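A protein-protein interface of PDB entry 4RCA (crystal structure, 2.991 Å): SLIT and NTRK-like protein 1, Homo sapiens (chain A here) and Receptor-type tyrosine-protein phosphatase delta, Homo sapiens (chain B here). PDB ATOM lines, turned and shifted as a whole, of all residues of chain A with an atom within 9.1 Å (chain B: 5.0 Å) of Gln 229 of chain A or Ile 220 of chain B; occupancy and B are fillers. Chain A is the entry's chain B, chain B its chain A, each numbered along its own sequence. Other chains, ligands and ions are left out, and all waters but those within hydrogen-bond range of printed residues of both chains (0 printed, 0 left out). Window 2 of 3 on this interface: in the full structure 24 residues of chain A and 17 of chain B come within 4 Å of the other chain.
The side-chain hydroxyl of Ser 219 of chain B sits close to the side-chain amide nitrogen of Gln 229 of chain A. NE of Arg 266 of chain B is in hydrogen-bond range of O of Gln 229 of chain A.
The side-chain hydroxyl of Ser 219 of chain B lies within hydrogen-bond range of the backbone carbonyl oxygen of Val 238 of chain B (3.0 Å). O of Ile 220 of chain B is in hydrogen-bond range of N of Val 238 of chain B. The backbone carbonyl oxygen of Cys 222 of chain A sits at hydrogen-bond distance from the backbone NH of Gly 230 of chain A (2.8 Å). N of Cys 222 of chain A lies within hydrogen-bond range of O of Lys 231 of chain A (3.0 Å). OD2 of Asp 240 of chain A is in salt-bridge range of NH2 of Arg 227 of chain A (2.5 Å). SG of Cys 197 of chain A forms a disulfide with SG of Cys 222 of chain A (2.0 Å).
Among the printed residues, merely in contact across the chains: Gly 230 of chain A with Arg 266 of chain B (3.4 Å), Arg 227 of chain A with Arg 266 of chain B (3.8 Å), Lys 231 of chain A with Arg 266 of chain B (3.8 Å), Thr 226 of chain A with Ile 220 of chain B (3.8 Å), Gln 229 of chain A with Val 238 of chain B (3.9 Å) and Gln 229 of chain A with Ile 220 of chain B (3.99 Å).
Cys 222 of chain A touches none of the printed residues of chain B. Of the printed residues of chain B, Thr 226 of chain A touches Ile 220 (3.8 Å). Of the printed residues of chain B, Arg 227 of chain A touches Arg 266 (3.8 Å). Of the printed residues of chain B, Gln 229 of chain A touches Ser 219, Ile 220, Val 238 and Arg 266. Of the printed residues of chain B, Gly 230 of chain A touches Arg 266. Printed residues of chain B within 4 Å of Lys 231 of chain A: Arg 266 (3.8 Å). Ser 219 of chain B touches just one residue of chain A: Gln 229. Printed residues of chain A within 4 Å of Ile 220 of chain B: Thr 226 and Gln 229. No residue of chain A comes within 4 Å of Pro 221 of chain B. Pro 222 of chain B touches none of the printed residues of chain A. No residue of chain A comes within 4 Å of Cys 237 of chain B. Of the printed residues of chain A, Arg 266 of chain B touches Arg 227 (3.8 Å), Gln 229 (2.9 Å), Gly 230 (3.4 Å) and Lys 231 (3.8 Å). The nearest printed residue of chain B that does not touch Gln 229 of chain A is Thr 236 of chain B (5.7 Å). The nearest printed residue of chain A that does not touch Ile 220 of chain B is Arg 227 of chain A (5.9 Å).
Of the 9 printed residues of chain B, 4 touch a printed residue of chain A. Printed residues of chain B that touch a printed residue of chain A: Ser 219, Ile 220, Val 238 and Arg 266. Along chain B the printed residues that touch a printed residue of chain A span positions 219 to 266.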
ATOM      1  N   TRP A 195     -19.806  24.222  18.481  1.00  0.00           N
ATOM      2  CA  TRP A 195     -21.180  23.822  18.752  1.00  0.00           C
ATOM      3  C   TRP A 195     -21.852  24.743  19.759  1.00  0.00           C
ATOM      4  O   TRP A 195     -21.372  24.923  20.879  1.00  0.00           O
ATOM      5  CB  TRP A 195     -21.226  22.377  19.247  1.00  0.00           C
ATOM      6  CG  TRP A 195     -20.809  21.396  18.203  1.00  0.00           C
ATOM      7  CD1 TRP A 195     -19.674  20.640  18.195  1.00  0.00           C
ATOM      8  CD2 TRP A 195     -21.513  21.077  16.999  1.00  0.00           C
ATOM      9  NE1 TRP A 195     -19.634  19.862  17.064  1.00  0.00           N
ATOM     10  CE2 TRP A 195     -20.752  20.113  16.312  1.00  0.00           C
ATOM     11  CE3 TRP A 195     -22.718  21.512  16.437  1.00  0.00           C
ATOM     12  CZ2 TRP A 195     -21.155  19.576  15.092  1.00  0.00           C
ATOM     13  CZ3 TRP A 195     -23.116  20.978  15.227  1.00  0.00           C
ATOM     14  CH2 TRP A 195     -22.337  20.018  14.568  1.00  0.00           C
ATOM     15  N   ASP A 196     -22.966  25.331  19.334  1.00  0.00           N
ATOM     16  CA  ASP A 196     -23.751  26.216  20.180  1.00  0.00           C
ATOM     17  C   ASP A 196     -24.882  25.426  20.825  1.00  0.00           C
ATOM     18  O   ASP A 196     -25.944  25.242  20.229  1.00  0.00           O
ATOM     19  CB  ASP A 196     -24.302  27.388  19.362  1.00  0.00           C
ATOM     20  CG  ASP A 196     -24.849  28.504  20.229  1.00  0.00           C
ATOM     21  OD1 ASP A 196     -24.521  28.549  21.434  1.00  0.00           O
ATOM     22  OD2 ASP A 196     -25.601  29.349  19.698  1.00  0.00           O
ATOM     23  N   CYS A 197     -24.645  24.948  22.040  1.00  0.00           N
ATOM     24  CA  CYS A 197     -25.630  24.123  22.725  1.00  0.00           C
ATOM     25  C   CYS A 197     -26.768  24.969  23.283  1.00  0.00           C
ATOM     26  O   CYS A 197     -26.670  25.546  24.369  1.00  0.00           O
ATOM     27  CB  CYS A 197     -24.967  23.320  23.834  1.00  0.00           C
ATOM     28  SG  CYS A 197     -23.442  22.483  23.349  1.00  0.00           S
ATOM     29  N   ARG A 219     -15.656  13.659  19.836  1.00  0.00           N
ATOM     30  CA  ARG A 219     -16.547  14.282  20.803  1.00  0.00           C
ATOM     31  C   ARG A 219     -17.251  15.505  20.228  1.00  0.00           C
ATOM     32  O   ARG A 219     -16.730  16.168  19.331  1.00  0.00           O
ATOM     33  CB  ARG A 219     -15.764  14.677  22.056  1.00  0.00           C
ATOM     34  CG  ARG A 219     -16.231  14.001  23.331  1.00  0.00           C
ATOM     35  CD  ARG A 219     -15.093  13.911  24.337  1.00  0.00           C
ATOM     36  NE  ARG A 219     -14.400  15.186  24.494  1.00  0.00           N
ATOM     37  CZ  ARG A 219     -14.324  15.868  25.633  1.00  0.00           C
ATOM     38  NH1 ARG A 219     -14.899  15.398  26.732  1.00  0.00           N
ATOM     39  NH2 ARG A 219     -13.672  17.021  25.673  1.00  0.00           N
ATOM     40  N   VAL A 221     -18.242  18.815  21.794  1.00  0.00           N
ATOM     41  CA  VAL A 221     -18.122  19.663  22.971  1.00  0.00           C
ATOM     42  C   VAL A 221     -18.819  21.003  22.742  1.00  0.00           C
ATOM     43  O   VAL A 221     -18.761  21.562  21.647  1.00  0.00           O
ATOM     44  CB  VAL A 221     -16.638  19.895  23.332  1.00  0.00           C
ATOM     45  CG1 VAL A 221     -16.513  20.591  24.676  1.00  0.00           C
ATOM     46  CG2 VAL A 221     -15.884  18.571  23.346  1.00  0.00           C
ATOM     47  N   CYS A 222     -19.488  21.505  23.777  1.00  0.00           N
ATOM     48  CA  CYS A 222     -20.148  22.806  23.716  1.00  0.00           C
ATOM     49  C   CYS A 222     -19.144  23.947  23.854  1.00  0.00           C
ATOM     50  O   CYS A 222     -18.476  24.069  24.877  1.00  0.00           O
ATOM     51  CB  CYS A 222     -21.211  22.923  24.812  1.00  0.00           C
ATOM     52  SG  CYS A 222     -22.414  21.575  24.845  1.00  0.00           S
ATOM     53  N   GLU A 223     -19.043  24.780  22.825  1.00  0.00           N
ATOM     54  CA  GLU A 223     -18.179  25.955  22.873  1.00  0.00           C
ATOM     55  C   GLU A 223     -18.962  27.142  23.428  1.00  0.00           C
ATOM     56  O   GLU A 223     -18.387  28.120  23.908  1.00  0.00           O
ATOM     57  CB  GLU A 223     -17.620  26.265  21.479  1.00  0.00           C
ATOM     58  CG  GLU A 223     -16.662  27.447  21.408  1.00  0.00           C
ATOM     59  CD  GLU A 223     -15.957  27.541  20.069  1.00  0.00           C
ATOM     60  OE1 GLU A 223     -15.503  26.493  19.562  1.00  0.00           O
ATOM     61  OE2 GLU A 223     -15.857  28.658  19.520  1.00  0.00           O
ATOM     62  N   ALA A 224     -20.285  27.029  23.376  1.00  0.00           N
ATOM     63  CA  ALA A 224     -21.176  28.097  23.809  1.00  0.00           C
ATOM     64  C   ALA A 224     -22.480  27.520  24.360  1.00  0.00           C
ATOM     65  O   ALA A 224     -22.925  26.463  23.914  1.00  0.00           O
ATOM     66  CB  ALA A 224     -21.456  29.048  22.654  1.00  0.00           C
ATOM     67  N   PRO A 225     -23.094  28.207  25.341  1.00  0.00           N
ATOM     68  CA  PRO A 225     -22.588  29.427  25.984  1.00  0.00           C
ATOM     69  C   PRO A 225     -21.483  29.141  27.002  1.00  0.00           C
ATOM     70  O   PRO A 225     -21.151  27.978  27.232  1.00  0.00           O
ATOM     71  CB  PRO A 225     -23.831  29.997  26.672  1.00  0.00           C
ATOM     72  CG  PRO A 225     -24.675  28.808  26.955  1.00  0.00           C
ATOM     73  CD  PRO A 225     -24.451  27.863  25.805  1.00  0.00           C
ATOM     74  N   THR A 226     -20.925  30.194  27.594  1.00  0.00           N
ATOM     75  CA  THR A 226     -19.882  30.054  28.609  1.00  0.00           C
ATOM     76  C   THR A 226     -20.399  29.307  29.833  1.00  0.00           C
ATOM     77  O   THR A 226     -19.624  28.732  30.598  1.00  0.00           O
ATOM     78  CB  THR A 226     -19.331  31.422  29.052  1.00  0.00           C
ATOM     79  OG1 THR A 226     -20.411  32.355  29.180  1.00  0.00           O
ATOM     80  CG2 THR A 226     -18.333  31.950  28.034  1.00  0.00           C
ATOM     81  N   ARG A 227     -21.715  29.328  30.008  1.00  0.00           N
ATOM     82  CA  ARG A 227     -22.379  28.558  31.051  1.00  0.00           C
ATOM     83  C   ARG A 227     -22.095  27.071  30.876  1.00  0.00           C
ATOM     84  O   ARG A 227     -22.083  26.306  31.842  1.00  0.00           O
ATOM     85  CB  ARG A 227     -23.889  28.808  31.013  1.00  0.00           C
ATOM     86  CG  ARG A 227     -24.579  28.706  32.358  1.00  0.00           C
ATOM     87  CD  ARG A 227     -26.082  28.542  32.201  1.00  0.00           C
ATOM     88  NE  ARG A 227     -26.472  27.136  32.178  1.00  0.00           N
ATOM     89  CZ  ARG A 227     -26.607  26.385  33.267  1.00  0.00           C
ATOM     90  NH1 ARG A 227     -26.379  26.906  34.466  1.00  0.00           N
ATOM     91  NH2 ARG A 227     -26.965  25.114  33.159  1.00  0.00           N
ATOM     92  N   LEU A 228     -21.856  26.676  29.630  1.00  0.00           N
ATOM     93  CA  LEU A 228     -21.770  25.269  29.263  1.00  0.00           C
ATOM     94  C   LEU A 228     -20.454  24.909  28.579  1.00  0.00           C
ATOM     95  O   LEU A 228     -20.191  23.738  28.297  1.00  0.00           O
ATOM     96  CB  LEU A 228     -22.938  24.913  28.347  1.00  0.00           C
ATOM     97  CG  LEU A 228     -23.124  23.436  28.017  1.00  0.00           C
ATOM     98  CD1 LEU A 228     -23.303  22.609  29.285  1.00  0.00           C
ATOM     99  CD2 LEU A 228     -24.290  23.283  27.098  1.00  0.00           C
ATOM    100  N   GLN A 229     -19.631  25.918  28.317  1.00  0.00           N
ATOM    101  CA  GLN A 229     -18.396  25.728  27.565  1.00  0.00           C
ATOM    102  C   GLN A 229     -17.524  24.616  28.139  1.00  0.00           C
ATOM    103  O   GLN A 229     -17.329  24.527  29.351  1.00  0.00           O
ATOM    104  CB  GLN A 229     -17.603  27.032  27.512  1.00  0.00           C
ATOM    105  CG  GLN A 229     -16.388  26.971  26.605  1.00  0.00           C
ATOM    106  CD  GLN A 229     -15.684  28.304  26.496  1.00  0.00           C
ATOM    107  OE1 GLN A 229     -16.257  29.347  26.812  1.00  0.00           O
ATOM    108  NE2 GLN A 229     -14.433  28.280  26.052  1.00  0.00           N
ATOM    109  N   GLY A 230     -17.019  23.761  27.254  1.00  0.00           N
ATOM    110  CA  GLY A 230     -16.150  22.669  27.648  1.00  0.00           C
ATOM    111  C   GLY A 230     -16.868  21.393  28.045  1.00  0.00           C
ATOM    112  O   GLY A 230     -16.223  20.398  28.383  1.00  0.00           O
ATOM    113  N   LYS A 231     -18.197  21.407  28.000  1.00  0.00           N
ATOM    114  CA  LYS A 231     -18.969  20.256  28.457  1.00  0.00           C
ATOM    115  C   LYS A 231     -19.435  19.377  27.300  1.00  0.00           C
ATOM    116  O   LYS A 231     -19.794  19.873  26.233  1.00  0.00           O
ATOM    117  CB  LYS A 231     -20.175  20.713  29.282  1.00  0.00           C
ATOM    118  CG  LYS A 231     -20.458  19.840  30.499  1.00  0.00           C
ATOM    119  CD  LYS A 231     -21.908  19.957  30.954  1.00  0.00           C
ATOM    120  CE  LYS A 231     -22.031  20.591  32.340  1.00  0.00           C
ATOM    121  NZ  LYS A 231     -22.336  19.601  33.412  1.00  0.00           N
ATOM    122  N   ASP A 232     -19.422  18.067  27.528  1.00  0.00           N
ATOM    123  CA  ASP A 232     -19.858  17.091  26.537  1.00  0.00           C
ATOM    124  C   ASP A 232     -21.377  17.115  26.349  1.00  0.00           C
ATOM    125  O   ASP A 232     -22.138  17.277  27.313  1.00  0.00           O
ATOM    126  CB  ASP A 232     -19.386  15.686  26.943  1.00  0.00           C
ATOM    127  CG  ASP A 232     -18.012  15.336  26.377  1.00  0.00           C
ATOM    128  OD1 ASP A 232     -17.213  16.255  26.103  1.00  0.00           O
ATOM    129  OD2 ASP A 232     -17.736  14.128  26.201  1.00  0.00           O
ATOM    130  N   THR A 236     -25.276  16.335  28.881  1.00  0.00           N
ATOM    131  CA  THR A 236     -25.897  17.645  29.004  1.00  0.00           C
ATOM    132  C   THR A 236     -27.391  17.493  29.239  1.00  0.00           C
ATOM    133  O   THR A 236     -28.105  16.977  28.382  1.00  0.00           O
ATOM    134  CB  THR A 236     -25.700  18.525  27.757  1.00  0.00           C
ATOM    135  OG1 THR A 236     -24.332  18.483  27.328  1.00  0.00           O
ATOM    136  CG2 THR A 236     -26.092  19.959  28.079  1.00  0.00           C
ATOM    137  N   ASP A 240     -30.527  22.362  30.464  1.00  0.00           N
ATOM    138  CA  ASP A 240     -29.394  23.241  30.235  1.00  0.00           C
ATOM    139  C   ASP A 240     -29.339  23.717  28.781  1.00  0.00           C
ATOM    140  O   ASP A 240     -29.000  24.872  28.511  1.00  0.00           O
ATOM    141  CB  ASP A 240     -28.101  22.534  30.630  1.00  0.00           C
ATOM    142  CG  ASP A 240     -26.879  23.269  30.162  1.00  0.00           C
ATOM    143  OD1 ASP A 240     -26.488  23.042  29.004  1.00  0.00           O
ATOM    144  OD2 ASP A 240     -26.315  24.069  30.941  1.00  0.00           O
ATOM    145  N   PHE B 218      -5.986  28.637  28.905  1.00  0.00           N
ATOM    146  CA  PHE B 218      -7.168  28.697  29.754  1.00  0.00           C
ATOM    147  C   PHE B 218      -8.287  29.502  29.105  1.00  0.00           C
ATOM    148  O   PHE B 218      -8.291  30.732  29.161  1.00  0.00           O
ATOM    149  CB  PHE B 218      -6.825  29.300  31.119  1.00  0.00           C
ATOM    150  CG  PHE B 218      -6.113  28.352  32.040  1.00  0.00           C
ATOM    151  CD1 PHE B 218      -6.750  27.217  32.512  1.00  0.00           C
ATOM    152  CD2 PHE B 218      -4.811  28.601  32.443  1.00  0.00           C
ATOM    153  CE1 PHE B 218      -6.100  26.341  33.361  1.00  0.00           C
ATOM    154  CE2 PHE B 218      -4.156  27.730  33.294  1.00  0.00           C
ATOM    155  CZ  PHE B 218      -4.802  26.598  33.752  1.00  0.00           C
ATOM    156  N   SER B 219      -9.232  28.798  28.490  1.00  0.00           N
ATOM    157  CA  SER B 219     -10.418  29.434  27.932  1.00  0.00           C
ATOM    158  C   SER B 219     -11.265  30.041  29.051  1.00  0.00           C
ATOM    159  O   SER B 219     -11.704  31.190  28.955  1.00  0.00           O
ATOM    160  CB  SER B 219     -11.239  28.427  27.123  1.00  0.00           C
ATOM    161  OG  SER B 219     -11.708  27.375  27.945  1.00  0.00           O
ATOM    162  N   ILE B 220     -11.495  29.266  30.109  1.00  0.00           N
ATOM    163  CA  ILE B 220     -12.118  29.799  31.318  1.00  0.00           C
ATOM    164  C   ILE B 220     -11.190  29.620  32.518  1.00  0.00           C
ATOM    165  O   ILE B 220     -11.052  28.512  33.044  1.00  0.00           O
ATOM    166  CB  ILE B 220     -13.471  29.126  31.621  1.00  0.00           C
ATOM    167  CG1 ILE B 220     -14.463  29.402  30.493  1.00  0.00           C
ATOM    168  CG2 ILE B 220     -14.033  29.632  32.938  1.00  0.00           C
ATOM    169  CD1 ILE B 220     -15.852  28.871  30.749  1.00  0.00           C
ATOM    170  N   PRO B 221     -10.539  30.712  32.951  1.00  0.00           N
ATOM    171  CA  PRO B 221      -9.623  30.641  34.094  1.00  0.00           C
ATOM    172  C   PRO B 221     -10.365  30.485  35.418  1.00  0.00           C
ATOM    173  O   PRO B 221     -11.514  30.912  35.526  1.00  0.00           O
ATOM    174  CB  PRO B 221      -8.881  31.985  34.042  1.00  0.00           C
ATOM    175  CG  PRO B 221      -9.171  32.547  32.676  1.00  0.00           C
ATOM    176  CD  PRO B 221     -10.529  32.046  32.329  1.00  0.00           C
ATOM    177  N   PRO B 222      -9.716  29.870  36.416  1.00  0.00           N
ATOM    178  CA  PRO B 222     -10.332  29.731  37.740  1.00  0.00           C
ATOM    179  C   PRO B 222     -10.453  31.076  38.451  1.00  0.00           C
ATOM    180  O   PRO B 222      -9.445  31.737  38.698  1.00  0.00           O
ATOM    181  CB  PRO B 222      -9.369  28.797  38.478  1.00  0.00           C
ATOM    182  CG  PRO B 222      -8.059  28.990  37.795  1.00  0.00           C
ATOM    183  CD  PRO B 222      -8.386  29.239  36.352  1.00  0.00           C
ATOM    184  N   THR B 236     -15.093  26.883  38.229  1.00  0.00           N
ATOM    185  CA  THR B 236     -15.018  26.330  36.883  1.00  0.00           C
ATOM    186  C   THR B 236     -13.663  26.589  36.234  1.00  0.00           C
ATOM    187  O   THR B 236     -13.265  27.736  36.055  1.00  0.00           O
ATOM    188  CB  THR B 236     -16.115  26.918  35.989  1.00  0.00           C
ATOM    189  OG1 THR B 236     -17.398  26.498  36.469  1.00  0.00           O
ATOM    190  CG2 THR B 236     -15.937  26.462  34.549  1.00  0.00           C
ATOM    191  N   CYS B 237     -12.959  25.520  35.876  1.00  0.00           N
ATOM    192  CA  CYS B 237     -11.696  25.649  35.158  1.00  0.00           C
ATOM    193  C   CYS B 237     -11.779  24.934  33.814  1.00  0.00           C
ATOM    194  O   CYS B 237     -12.021  23.731  33.762  1.00  0.00           O
ATOM    195  CB  CYS B 237     -10.540  25.092  35.989  1.00  0.00           C
ATOM    196  SG  CYS B 237      -8.924  25.206  35.192  1.00  0.00           S
ATOM    197  N   VAL B 238     -11.592  25.680  32.730  1.00  0.00           N
ATOM    198  CA  VAL B 238     -11.678  25.116  31.381  1.00  0.00           C
ATOM    199  C   VAL B 238     -10.466  25.509  30.534  1.00  0.00           C
ATOM    200  O   VAL B 238     -10.153  26.695  30.404  1.00  0.00           O
ATOM    201  CB  VAL B 238     -12.961  25.575  30.652  1.00  0.00           C
ATOM    202  CG1 VAL B 238     -13.102  24.857  29.321  1.00  0.00           C
ATOM    203  CG2 VAL B 238     -14.192  25.335  31.518  1.00  0.00           C
ATOM    204  N   ARG B 266     -12.275  20.175  30.744  1.00  0.00           N
ATOM    205  CA  ARG B 266     -13.055  20.902  31.743  1.00  0.00           C
ATOM    206  C   ARG B 266     -13.122  20.223  33.114  1.00  0.00           C
ATOM    207  O   ARG B 266     -13.327  19.015  33.214  1.00  0.00           O
ATOM    208  CB  ARG B 266     -14.474  21.120  31.213  1.00  0.00           C
ATOM    209  CG  ARG B 266     -15.411  21.855  32.160  1.00  0.00           C
ATOM    210  CD  ARG B 266     -16.831  21.882  31.603  1.00  0.00           C
ATOM    211  NE  ARG B 266     -17.517  23.137  31.899  1.00  0.00           N
ATOM    212  CZ  ARG B 266     -18.468  23.285  32.818  1.00  0.00           C
ATOM    213  NH1 ARG B 266     -18.873  22.251  33.543  1.00  0.00           N
ATOM    214  NH2 ARG B 266     -19.023  24.475  33.005  1.00  0.00           N
